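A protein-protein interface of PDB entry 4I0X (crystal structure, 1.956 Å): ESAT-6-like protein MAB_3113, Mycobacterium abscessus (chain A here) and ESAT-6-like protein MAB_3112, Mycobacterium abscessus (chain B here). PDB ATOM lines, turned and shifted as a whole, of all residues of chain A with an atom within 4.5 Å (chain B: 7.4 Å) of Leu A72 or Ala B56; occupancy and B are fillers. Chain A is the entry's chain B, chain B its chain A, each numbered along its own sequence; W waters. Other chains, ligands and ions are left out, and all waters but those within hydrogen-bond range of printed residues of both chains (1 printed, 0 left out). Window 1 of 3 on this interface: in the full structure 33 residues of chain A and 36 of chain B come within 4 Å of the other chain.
The side-chain carboxylate of Asp B54 is in salt-bridge range of the side-chain amino group of Lys B58 (3.0 Å).
The side-chain carboxylate (OE1) of Glu A74 sits close to the side-chain carboxylate (OE2) of Glu B51 (2.9 Å).
The backbone carbonyl oxygen (O) of Glu B51 sits close to the side-chain carboxylate (OE1) of Glu A71, 3.5 Å away.
The side-chain carboxylate (OD2) of Asp B54 lies close to the side-chain carboxylate (OE1) of Glu A71.
The side-chain amino group (NZ) of Lys B58 lies within salt-bridge range of the side-chain carboxylate (OE2) of Glu A71 (2.9 Å).
Water W1 bridges the side-chain carboxylate of Glu A71 and the side-chain amino group of Lys B58.
Leu A72 touches just these residues of chain B: Met B52 and Ala B56.
Ala B16 touches none of the printed residues of chain A.
Printed residues of chain A within 4 Å of Gly B48: Gly A75.
Of the printed residues of chain A, Glu B51 touches Glu A71 (3.3 Å), Glu A74 (2.9 Å) and Gly A75 (3.96 Å).
Of the printed residues of chain A, Lys B58 touches Ala A68 (3.5 Å) and Glu A71 (2.9 Å).
Among the printed residues, pairs that only touch across the chains: Phe A26 with Met B19 (3.6 Å), Phe A26 with Gly B22 (3.9 Å), Phe A26 with Ser B23 (3.9 Å), Phe A26 with Leu B26 (3.6 Å), Ala A68 with Gly B55 (3.3 Å), Ala A68 with Lys B58 (3.5 Å), Ala A68 with Val B59 (3.4 Å), Ala A69 with Val B59 (3.9 Å), Glu A71 with Gly B55 (3.8 Å), Leu A72 with Met B52 (3.7 Å), Leu A72 with Ala B56 (3.95 Å), Gly A75 with Gly B48 (3.2 Å), Gly A75 with Glu B51 (3.96 Å), Gly A75 with Met B52 (3.99 Å) and Leu A76 with Met B52 (3.8 Å).
Hydrophobic or aromatic side chains of chain A that line the printed part of chain B: Phe A26, Ala A68, Leu A72 and Leu A76.
Along chain A the printed residues that touch a printed residue of chain B span positions 26 to 76.
Among the printed residues, Asp or Glu carboxylates within 4 Å of a Lys or Arg side-chain nitrogen of the other chain: Glu A71 with Lys B58 (2.9 Å).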
ATOM      1  N   PHE A  26     -26.575  22.645  -7.974  1.00  0.00           N
ATOM      2  CA  PHE A  26     -25.442  22.281  -7.134  1.00  0.00           C
ATOM      3  C   PHE A  26     -24.440  21.429  -7.922  1.00  0.00           C
ATOM      4  O   PHE A  26     -23.255  21.707  -7.899  1.00  0.00           O
ATOM      5  CB  PHE A  26     -25.925  21.526  -5.911  1.00  0.00           C
ATOM      6  CG  PHE A  26     -24.844  21.172  -4.958  1.00  0.00           C
ATOM      7  CD1 PHE A  26     -24.235  22.144  -4.192  1.00  0.00           C
ATOM      8  CD2 PHE A  26     -24.452  19.870  -4.808  1.00  0.00           C
ATOM      9  CE1 PHE A  26     -23.231  21.804  -3.289  1.00  0.00           C
ATOM     10  CE2 PHE A  26     -23.449  19.524  -3.892  1.00  0.00           C
ATOM     11  CZ  PHE A  26     -22.853  20.503  -3.135  1.00  0.00           C
ATOM     12  N   LYS A  27     -24.920  20.392  -8.604  1.00  0.00           N
ATOM     13  CA  LYS A  27     -24.052  19.585  -9.444  1.00  0.00           C
ATOM     14  C   LYS A  27     -23.295  20.430 -10.456  1.00  0.00           C
ATOM     15  O   LYS A  27     -22.123  20.202 -10.697  1.00  0.00           O
ATOM     16  CB  LYS A  27     -24.854  18.472 -10.151  1.00  0.00           C
ATOM     17  CG  LYS A  27     -24.041  17.596 -11.059  1.00  0.00           C
ATOM     18  CD  LYS A  27     -23.948  18.177 -12.452  1.00  0.00           C
ATOM     19  CE  LYS A  27     -24.315  17.158 -13.468  1.00  0.00           C
ATOM     20  NZ  LYS A  27     -24.160  17.686 -14.860  1.00  0.00           N
ATOM     21  N   ALA A  68     -15.912  10.700  -7.067  1.00  0.00           N
ATOM     22  CA  ALA A  68     -17.058  11.253  -6.320  1.00  0.00           C
ATOM     23  C   ALA A  68     -17.994  12.095  -7.188  1.00  0.00           C
ATOM     24  O   ALA A  68     -19.217  12.014  -7.065  1.00  0.00           O
ATOM     25  CB  ALA A  68     -16.578  12.058  -5.153  1.00  0.00           C
ATOM     26  N   ALA A  69     -17.424  12.930  -8.047  1.00  0.00           N
ATOM     27  CA  ALA A  69     -18.226  13.680  -9.005  1.00  0.00           C
ATOM     28  C   ALA A  69     -19.117  12.767  -9.845  1.00  0.00           C
ATOM     29  O   ALA A  69     -20.264  13.103 -10.062  1.00  0.00           O
ATOM     30  CB  ALA A  69     -17.349  14.518  -9.899  1.00  0.00           C
ATOM     31  N   ARG A  70     -18.593  11.620 -10.297  1.00  0.00           N
ATOM     32  CA  ARG A  70     -19.385  10.643 -11.054  1.00  0.00           C
ATOM     33  C   ARG A  70     -20.540  10.123 -10.195  1.00  0.00           C
ATOM     34  O   ARG A  70     -21.663   9.989 -10.663  1.00  0.00           O
ATOM     35  CB  ARG A  70     -18.512   9.476 -11.554  1.00  0.00           C
ATOM     36  CG  ARG A  70     -19.230   8.492 -12.511  1.00  0.00           C
ATOM     37  CD  ARG A  70     -18.259   7.510 -13.200  1.00  0.00           C
ATOM     38  NE  ARG A  70     -17.342   8.177 -14.137  1.00  0.00           N
ATOM     39  CZ  ARG A  70     -17.547   8.321 -15.450  1.00  0.00           C
ATOM     40  NH1 ARG A  70     -18.645   7.849 -16.025  1.00  0.00           N
ATOM     41  NH2 ARG A  70     -16.646   8.952 -16.194  1.00  0.00           N
ATOM     42  N   GLU A  71     -20.275   9.897  -8.917  1.00  0.00           N
ATOM     43  CA  GLU A  71     -21.283   9.370  -8.021  1.00  0.00           C
ATOM     44  C   GLU A  71     -22.306  10.447  -7.773  1.00  0.00           C
ATOM     45  O   GLU A  71     -23.502  10.203  -7.695  1.00  0.00           O
ATOM     46  CB  GLU A  71     -20.645   8.850  -6.712  1.00  0.00           C
ATOM     47  CG  GLU A  71     -21.669   8.437  -5.700  1.00  0.00           C
ATOM     48  CD  GLU A  71     -21.064   7.950  -4.413  1.00  0.00           C
ATOM     49  OE1 GLU A  71     -21.852   7.468  -3.559  1.00  0.00           O
ATOM     50  OE2 GLU A  71     -19.814   8.044  -4.269  1.00  0.00           O
ATOM     51  N   LEU A  72     -21.844  11.685  -7.775  1.00  0.00           N
ATOM     52  CA  LEU A  72     -22.740  12.779  -7.582  1.00  0.00           C
ATOM     53  C   LEU A  72     -23.710  12.951  -8.779  1.00  0.00           C
ATOM     54  O   LEU A  72     -24.919  13.194  -8.592  1.00  0.00           O
ATOM     55  CB  LEU A  72     -21.906  14.022  -7.313  1.00  0.00           C
ATOM     56  CG  LEU A  72     -22.658  15.222  -6.826  1.00  0.00           C
ATOM     57  CD1 LEU A  72     -21.736  16.062  -6.049  1.00  0.00           C
ATOM     58  CD2 LEU A  72     -23.181  15.948  -8.051  1.00  0.00           C
ATOM     59  N   VAL A  73     -23.201  12.781  -9.994  1.00  0.00           N
ATOM     60  CA  VAL A  73     -24.040  12.888 -11.176  1.00  0.00           C
ATOM     61  C   VAL A  73     -24.995  11.675 -11.321  1.00  0.00           C
ATOM     62  O   VAL A  73     -26.149  11.819 -11.748  1.00  0.00           O
ATOM     63  CB  VAL A  73     -23.228  13.076 -12.478  1.00  0.00           C
ATOM     64  CG1 VAL A  73     -22.171  14.167 -12.302  1.00  0.00           C
ATOM     65  CG2 VAL A  73     -22.572  11.794 -12.884  1.00  0.00           C
ATOM     66  N   GLU A  74     -24.529  10.485 -10.972  1.00  0.00           N
ATOM     67  CA  GLU A  74     -25.365   9.307 -11.081  1.00  0.00           C
ATOM     68  C   GLU A  74     -26.537   9.406 -10.086  1.00  0.00           C
ATOM     69  O   GLU A  74     -27.663   9.009 -10.388  1.00  0.00           O
ATOM     70  CB  GLU A  74     -24.564   8.017 -10.859  1.00  0.00           C
ATOM     71  CG  GLU A  74     -25.371   6.750 -11.219  1.00  0.00           C
ATOM     72  CD  GLU A  74     -24.773   5.453 -10.677  1.00  0.00           C
ATOM     73  OE1 GLU A  74     -23.636   5.478 -10.155  1.00  0.00           O
ATOM     74  OE2 GLU A  74     -25.453   4.406 -10.770  1.00  0.00           O
ATOM     75  N   GLY A  75     -26.263   9.935  -8.898  1.00  0.00           N
ATOM     76  CA  GLY A  75     -27.297  10.157  -7.913  1.00  0.00           C
ATOM     77  C   GLY A  75     -28.316  11.161  -8.407  1.00  0.00           C
ATOM     78  O   GLY A  75     -29.523  10.932  -8.351  1.00  0.00           O
ATOM     79  N   LEU A  76     -27.831  12.289  -8.894  1.00  0.00           N
ATOM     80  CA  LEU A  76     -28.727  13.270  -9.474  1.00  0.00           C
ATOM     81  C   LEU A  76     -29.595  12.672 -10.593  1.00  0.00           C
ATOM     82  O   LEU A  76     -30.786  12.988 -10.680  1.00  0.00           O
ATOM     83  CB  LEU A  76     -27.937  14.485  -9.977  1.00  0.00           C
ATOM     84  CG  LEU A  76     -28.742  15.488 -10.752  1.00  0.00           C
ATOM     85  CD1 LEU A  76     -29.704  16.169  -9.806  1.00  0.00           C
ATOM     86  CD2 LEU A  76     -27.827  16.501 -11.434  1.00  0.00           C
ATOM     87  N   ALA B  16     -14.694  23.787  -0.802  1.00  0.00           N
ATOM     88  CA  ALA B  16     -15.086  22.841   0.262  1.00  0.00           C
ATOM     89  C   ALA B  16     -16.149  23.446   1.188  1.00  0.00           C
ATOM     90  O   ALA B  16     -17.176  22.819   1.448  1.00  0.00           O
ATOM     91  CB  ALA B  16     -13.840  22.372   1.087  1.00  0.00           C
ATOM     92  N   MET B  19     -19.472  23.701  -0.713  1.00  0.00           N
ATOM     93  CA  MET B  19     -20.078  22.388  -0.958  1.00  0.00           C
ATOM     94  C   MET B  19     -20.699  21.787   0.273  1.00  0.00           C
ATOM     95  O   MET B  19     -21.781  21.166   0.210  1.00  0.00           O
ATOM     96  CB  MET B  19     -19.047  21.439  -1.547  1.00  0.00           C
ATOM     97  CG  MET B  19     -18.748  21.712  -2.985  1.00  0.00           C
ATOM     98  SD  MET B  19     -17.750  20.405  -3.729  1.00  0.00           S
ATOM     99  CE  MET B  19     -18.873  19.015  -3.463  1.00  0.00           C
ATOM    100  N   ARG B  20     -20.059  22.018   1.420  1.00  0.00           N
ATOM    101  CA  ARG B  20     -20.576  21.512   2.658  1.00  0.00           C
ATOM    102  C   ARG B  20     -21.899  22.178   2.969  1.00  0.00           C
ATOM    103  O   ARG B  20     -22.889  21.477   3.302  1.00  0.00           O
ATOM    104  CB  ARG B  20     -19.608  21.735   3.831  1.00  0.00           C
ATOM    105  CG  ARG B  20     -20.086  21.051   5.109  1.00  0.00           C
ATOM    106  CD  ARG B  20     -19.193  21.367   6.290  1.00  0.00           C
ATOM    107  NE  ARG B  20     -18.803  20.163   7.031  1.00  0.00           N
ATOM    108  CZ  ARG B  20     -19.586  19.473   7.867  1.00  0.00           C
ATOM    109  NH1 ARG B  20     -20.848  19.835   8.087  1.00  0.00           N
ATOM    110  NH2 ARG B  20     -19.097  18.399   8.482  1.00  0.00           N
ATOM    111  N   GLY B  22     -23.895  23.760   0.857  1.00  0.00           N
ATOM    112  CA  GLY B  22     -24.854  23.420  -0.172  1.00  0.00           C
ATOM    113  C   GLY B  22     -25.442  22.054   0.030  1.00  0.00           C
ATOM    114  O   GLY B  22     -26.645  21.849  -0.125  1.00  0.00           O
ATOM    115  N   SER B  23     -24.569  21.102   0.319  1.00  0.00           N
ATOM    116  CA  SER B  23     -24.977  19.751   0.607  1.00  0.00           C
ATOM    117  C   SER B  23     -25.926  19.643   1.818  1.00  0.00           C
ATOM    118  O   SER B  23     -26.905  18.908   1.778  1.00  0.00           O
ATOM    119  CB  SER B  23     -23.739  18.897   0.858  1.00  0.00           C
ATOM    120  OG  SER B  23     -24.122  17.546   1.025  1.00  0.00           O
ATOM    121  N   LEU B  26     -29.304  21.121   0.856  1.00  0.00           N
ATOM    122  CA  LEU B  26     -30.073  20.268  -0.037  1.00  0.00           C
ATOM    123  C   LEU B  26     -30.628  19.073   0.717  1.00  0.00           C
ATOM    124  O   LEU B  26     -31.683  18.596   0.411  1.00  0.00           O
ATOM    125  CB  LEU B  26     -29.208  19.759  -1.181  1.00  0.00           C
ATOM    126  CG  LEU B  26     -29.091  20.687  -2.359  1.00  0.00           C
ATOM    127  CD1 LEU B  26     -27.922  20.227  -3.199  1.00  0.00           C
ATOM    128  CD2 LEU B  26     -30.423  20.721  -3.155  1.00  0.00           C
ATOM    129  N   GLY B  48     -31.307   8.050  -4.701  1.00  0.00           N
ATOM    130  CA  GLY B  48     -30.535   8.932  -5.535  1.00  0.00           C
ATOM    131  C   GLY B  48     -29.828  10.028  -4.741  1.00  0.00           C
ATOM    132  O   GLY B  48     -28.653  10.309  -4.967  1.00  0.00           O
ATOM    133  N   TRP B  49     -30.565  10.657  -3.827  1.00  0.00           N
ATOM    134  CA  TRP B  49     -30.027  11.704  -2.975  1.00  0.00           C
ATOM    135  C   TRP B  49     -28.948  11.172  -2.033  1.00  0.00           C
ATOM    136  O   TRP B  49     -27.903  11.807  -1.853  1.00  0.00           O
ATOM    137  CB  TRP B  49     -31.126  12.461  -2.202  1.00  0.00           C
ATOM    138  CG  TRP B  49     -30.479  13.319  -1.189  1.00  0.00           C
ATOM    139  CD1 TRP B  49     -30.532  13.183   0.163  1.00  0.00           C
ATOM    140  CD2 TRP B  49     -29.599  14.414  -1.451  1.00  0.00           C
ATOM    141  NE1 TRP B  49     -29.752  14.144   0.762  1.00  0.00           N
ATOM    142  CE2 TRP B  49     -29.155  14.899  -0.209  1.00  0.00           C
ATOM    143  CE3 TRP B  49     -29.130  15.012  -2.609  1.00  0.00           C
ATOM    144  CZ2 TRP B  49     -28.275  15.968  -0.101  1.00  0.00           C
ATOM    145  CZ3 TRP B  49     -28.269  16.083  -2.501  1.00  0.00           C
ATOM    146  CH2 TRP B  49     -27.854  16.551  -1.255  1.00  0.00           C
ATOM    147  N   ASP B  50     -29.179  10.003  -1.460  1.00  0.00           N
ATOM    148  CA  ASP B  50     -28.187   9.343  -0.635  1.00  0.00           C
ATOM    149  C   ASP B  50     -26.896   9.152  -1.404  1.00  0.00           C
ATOM    150  O   ASP B  50     -25.817   9.391  -0.862  1.00  0.00           O
ATOM    151  CB  ASP B  50     -28.689   7.995  -0.172  1.00  0.00           C
ATOM    152  CG  ASP B  50     -29.784   8.105   0.881  1.00  0.00           C
ATOM    153  OD1 ASP B  50     -30.080   9.235   1.338  1.00  0.00           O
ATOM    154  OD2 ASP B  50     -30.336   7.043   1.257  1.00  0.00           O
ATOM    155  N   GLU B  51     -27.002   8.740  -2.666  1.00  0.00           N
ATOM    156  CA  GLU B  51     -25.811   8.593  -3.499  1.00  0.00           C
ATOM    157  C   GLU B  51     -25.216   9.964  -3.859  1.00  0.00           C
ATOM    158  O   GLU B  51     -24.030  10.146  -3.808  1.00  0.00           O
ATOM    159  CB  GLU B  51     -26.089   7.754  -4.751  1.00  0.00           C
ATOM    160  CG  GLU B  51     -24.917   7.766  -5.700  1.00  0.00           C
ATOM    161  CD  GLU B  51     -25.029   6.779  -6.849  1.00  0.00           C
ATOM    162  OE1 GLU B  51     -26.085   6.126  -7.022  1.00  0.00           O
ATOM    163  OE2 GLU B  51     -24.046   6.682  -7.598  1.00  0.00           O
ATOM    164  N   MET B  52     -26.038  10.945  -4.212  1.00  0.00           N
ATOM    165  CA  MET B  52     -25.530  12.289  -4.439  1.00  0.00           C
ATOM    166  C   MET B  52     -24.771  12.918  -3.210  1.00  0.00           C
ATOM    167  O   MET B  52     -23.694  13.509  -3.339  1.00  0.00           O
ATOM    168  CB  MET B  52     -26.699  13.169  -4.882  1.00  0.00           C
ATOM    169  CG  MET B  52     -26.319  14.498  -5.319  1.00  0.00           C
ATOM    170  SD  MET B  52     -27.618  15.374  -6.249  1.00  0.00           S
ATOM    171  CE  MET B  52     -26.532  16.690  -6.741  1.00  0.00           C
ATOM    172  N   GLN B  53     -25.350  12.812  -2.026  1.00  0.00           N
ATOM    173  CA  GLN B  53     -24.781  13.349  -0.821  1.00  0.00           C
ATOM    174  C   GLN B  53     -23.482  12.604  -0.491  1.00  0.00           C
ATOM    175  O   GLN B  53     -22.521  13.196  -0.012  1.00  0.00           O
ATOM    176  CB  GLN B  53     -25.785  13.179   0.303  1.00  0.00           C
ATOM    177  CG  GLN B  53     -25.372  13.757   1.614  1.00  0.00           C
ATOM    178  CD  GLN B  53     -26.410  13.484   2.685  1.00  0.00           C
ATOM    179  OE1 GLN B  53     -26.872  12.351   2.848  1.00  0.00           O
ATOM    180  NE2 GLN B  53     -26.806  14.525   3.403  1.00  0.00           N
ATOM    181  N   ASP B  54     -23.457  11.305  -0.744  1.00  0.00           N
ATOM    182  CA  ASP B  54     -22.249  10.532  -0.531  1.00  0.00           C
ATOM    183  C   ASP B  54     -21.149  11.063  -1.449  1.00  0.00           C
ATOM    184  O   ASP B  54     -20.022  11.235  -1.018  1.00  0.00           O
ATOM    185  CB  ASP B  54     -22.517   9.027  -0.727  1.00  0.00           C
ATOM    186  CG  ASP B  54     -21.308   8.143  -0.373  1.00  0.00           C
ATOM    187  OD1 ASP B  54     -20.924   8.087   0.832  1.00  0.00           O
ATOM    188  OD2 ASP B  54     -20.781   7.454  -1.293  1.00  0.00           O
ATOM    189  N   GLY B  55     -21.484  11.369  -2.700  1.00  0.00           N
ATOM    190  CA  GLY B  55     -20.490  11.868  -3.622  1.00  0.00           C
ATOM    191  C   GLY B  55     -19.973  13.229  -3.181  1.00  0.00           C
ATOM    192  O   GLY B  55     -18.776  13.514  -3.193  1.00  0.00           O
ATOM    193  N   ALA B  56     -20.889  14.057  -2.749  1.00  0.00           N
ATOM    194  CA  ALA B  56     -20.589  15.412  -2.308  1.00  0.00           C
ATOM    195  C   ALA B  56     -19.645  15.401  -1.117  1.00  0.00           C
ATOM    196  O   ALA B  56     -18.650  16.109  -1.101  1.00  0.00           O
ATOM    197  CB  ALA B  56     -21.894  16.167  -1.992  1.00  0.00           C
ATOM    198  N   THR B  57     -19.914  14.537  -0.150  1.00  0.00           N
ATOM    199  CA  THR B  57     -19.012  14.331   0.986  1.00  0.00           C
ATOM    200  C   THR B  57     -17.579  13.907   0.599  1.00  0.00           C
ATOM    201  O   THR B  57     -16.592  14.433   1.126  1.00  0.00           O
ATOM    202  CB  THR B  57     -19.614  13.286   1.929  1.00  0.00           C
ATOM    203  OG1 THR B  57     -20.923  13.733   2.300  1.00  0.00           O
ATOM    204  CG2 THR B  57     -18.753  13.078   3.178  1.00  0.00           C
ATOM    205  N   LYS B  58     -17.470  12.933  -0.295  1.00  0.00           N
ATOM    206  CA  LYS B  58     -16.171  12.493  -0.772  1.00  0.00           C
ATOM    207  C   LYS B  58     -15.450  13.657  -1.491  1.00  0.00           C
ATOM    208  O   LYS B  58     -14.236  13.820  -1.360  1.00  0.00           O
ATOM    209  CB  LYS B  58     -16.321  11.297  -1.711  1.00  0.00           C
ATOM    210  CG  LYS B  58     -16.888  10.051  -1.042  1.00  0.00           C
ATOM    211  CD  LYS B  58     -16.924   8.831  -1.982  1.00  0.00           C
ATOM    212  CE  LYS B  58     -17.931   7.802  -1.464  1.00  0.00           C
ATOM    213  NZ  LYS B  58     -18.111   6.610  -2.340  1.00  0.00           N
ATOM    214  N   VAL B  59     -16.188  14.447  -2.264  1.00  0.00           N
ATOM    215  CA  VAL B  59     -15.560  15.607  -2.920  1.00  0.00           C
ATOM    216  C   VAL B  59     -15.015  16.603  -1.875  1.00  0.00           C
ATOM    217  O   VAL B  59     -13.889  17.068  -1.961  1.00  0.00           O
ATOM    218  CB  VAL B  59     -16.544  16.334  -3.881  1.00  0.00           C
ATOM    219  CG1 VAL B  59     -15.969  17.688  -4.331  1.00  0.00           C
ATOM    220  CG2 VAL B  59     -16.874  15.472  -5.078  1.00  0.00           C
ATOM    221  N   TRP B  60     -15.834  16.891  -0.872  1.00  0.00           N
ATOM    222  CA  TRP B  60     -15.527  17.868   0.170  1.00  0.00           C
ATOM    223  C   TRP B  60     -14.295  17.423   0.918  1.00  0.00           C
ATOM    224  O   TRP B  60     -13.422  18.223   1.209  1.00  0.00           O
ATOM    225  CB  TRP B  60     -16.705  17.981   1.178  1.00  0.00           C
ATOM    226  CG  TRP B  60     -16.372  18.774   2.429  1.00  0.00           C
ATOM    227  CD1 TRP B  60     -16.552  20.117   2.610  1.00  0.00           C
ATOM    228  CD2 TRP B  60     -15.773  18.294   3.632  1.00  0.00           C
ATOM    229  NE1 TRP B  60     -16.114  20.507   3.853  1.00  0.00           N
ATOM    230  CE2 TRP B  60     -15.624  19.407   4.501  1.00  0.00           C
ATOM    231  CE3 TRP B  60     -15.331  17.044   4.064  1.00  0.00           C
ATOM    232  CZ2 TRP B  60     -15.068  19.295   5.770  1.00  0.00           C
ATOM    233  CZ3 TRP B  60     -14.773  16.940   5.338  1.00  0.00           C
ATOM    234  CH2 TRP B  60     -14.649  18.058   6.168  1.00  0.00           C
ATOM    235  N   ASN B  61     -14.226  16.138   1.213  1.00  0.00           N
ATOM    236  CA  ASN B  61     -13.072  15.561   1.890  1.00  0.00           C
ATOM    237  C   ASN B  61     -11.797  15.639   1.078  1.00  0.00           C
ATOM    238  O   ASN B  61     -10.716  15.882   1.623  1.00  0.00           O
ATOM    239  CB  ASN B  61     -13.337  14.118   2.296  1.00  0.00           C
ATOM    240  CG  ASN B  61     -14.026  14.024   3.658  1.00  0.00           C
ATOM    241  OD1 ASN B  61     -13.416  14.272   4.695  1.00  0.00           O
ATOM    242  ND2 ASN B  61     -15.292  13.680   3.653  1.00  0.00           N
ATOM    243  N   ALA B  62     -11.917  15.423  -0.221  1.00  0.00           N
ATOM    244  CA  ALA B  62     -10.744  15.469  -1.091  1.00  0.00           C
ATOM    245  C   ALA B  62     -10.252  16.903  -1.232  1.00  0.00           C
ATOM    246  O   ALA B  62      -9.046  17.142  -1.204  1.00  0.00           O
ATOM    247  CB  ALA B  62     -11.050  14.870  -2.454  1.00  0.00           C
ATOM    248  N   LEU B  63     -11.178  17.842  -1.351  1.00  0.00           N
ATOM    249  CA  LEU B  63     -10.845  19.269  -1.426  1.00  0.00           C
ATOM    250  C   LEU B  63     -10.147  19.787  -0.178  1.00  0.00           C
ATOM    251  O   LEU B  63      -9.177  20.483  -0.265  1.00  0.00           O
ATOM    252  CB  LEU B  63     -12.095  20.142  -1.684  1.00  0.00           C
ATOM    253  CG  LEU B  63     -12.647  20.021  -3.091  1.00  0.00           C
ATOM    254  CD1 LEU B  63     -14.009  20.627  -3.185  1.00  0.00           C
ATOM    255  CD2 LEU B  63     -11.704  20.650  -4.129  1.00  0.00           C
HETATM  256  O   HOH W   1     -17.312   7.494  -5.193  1.00  0.00           O
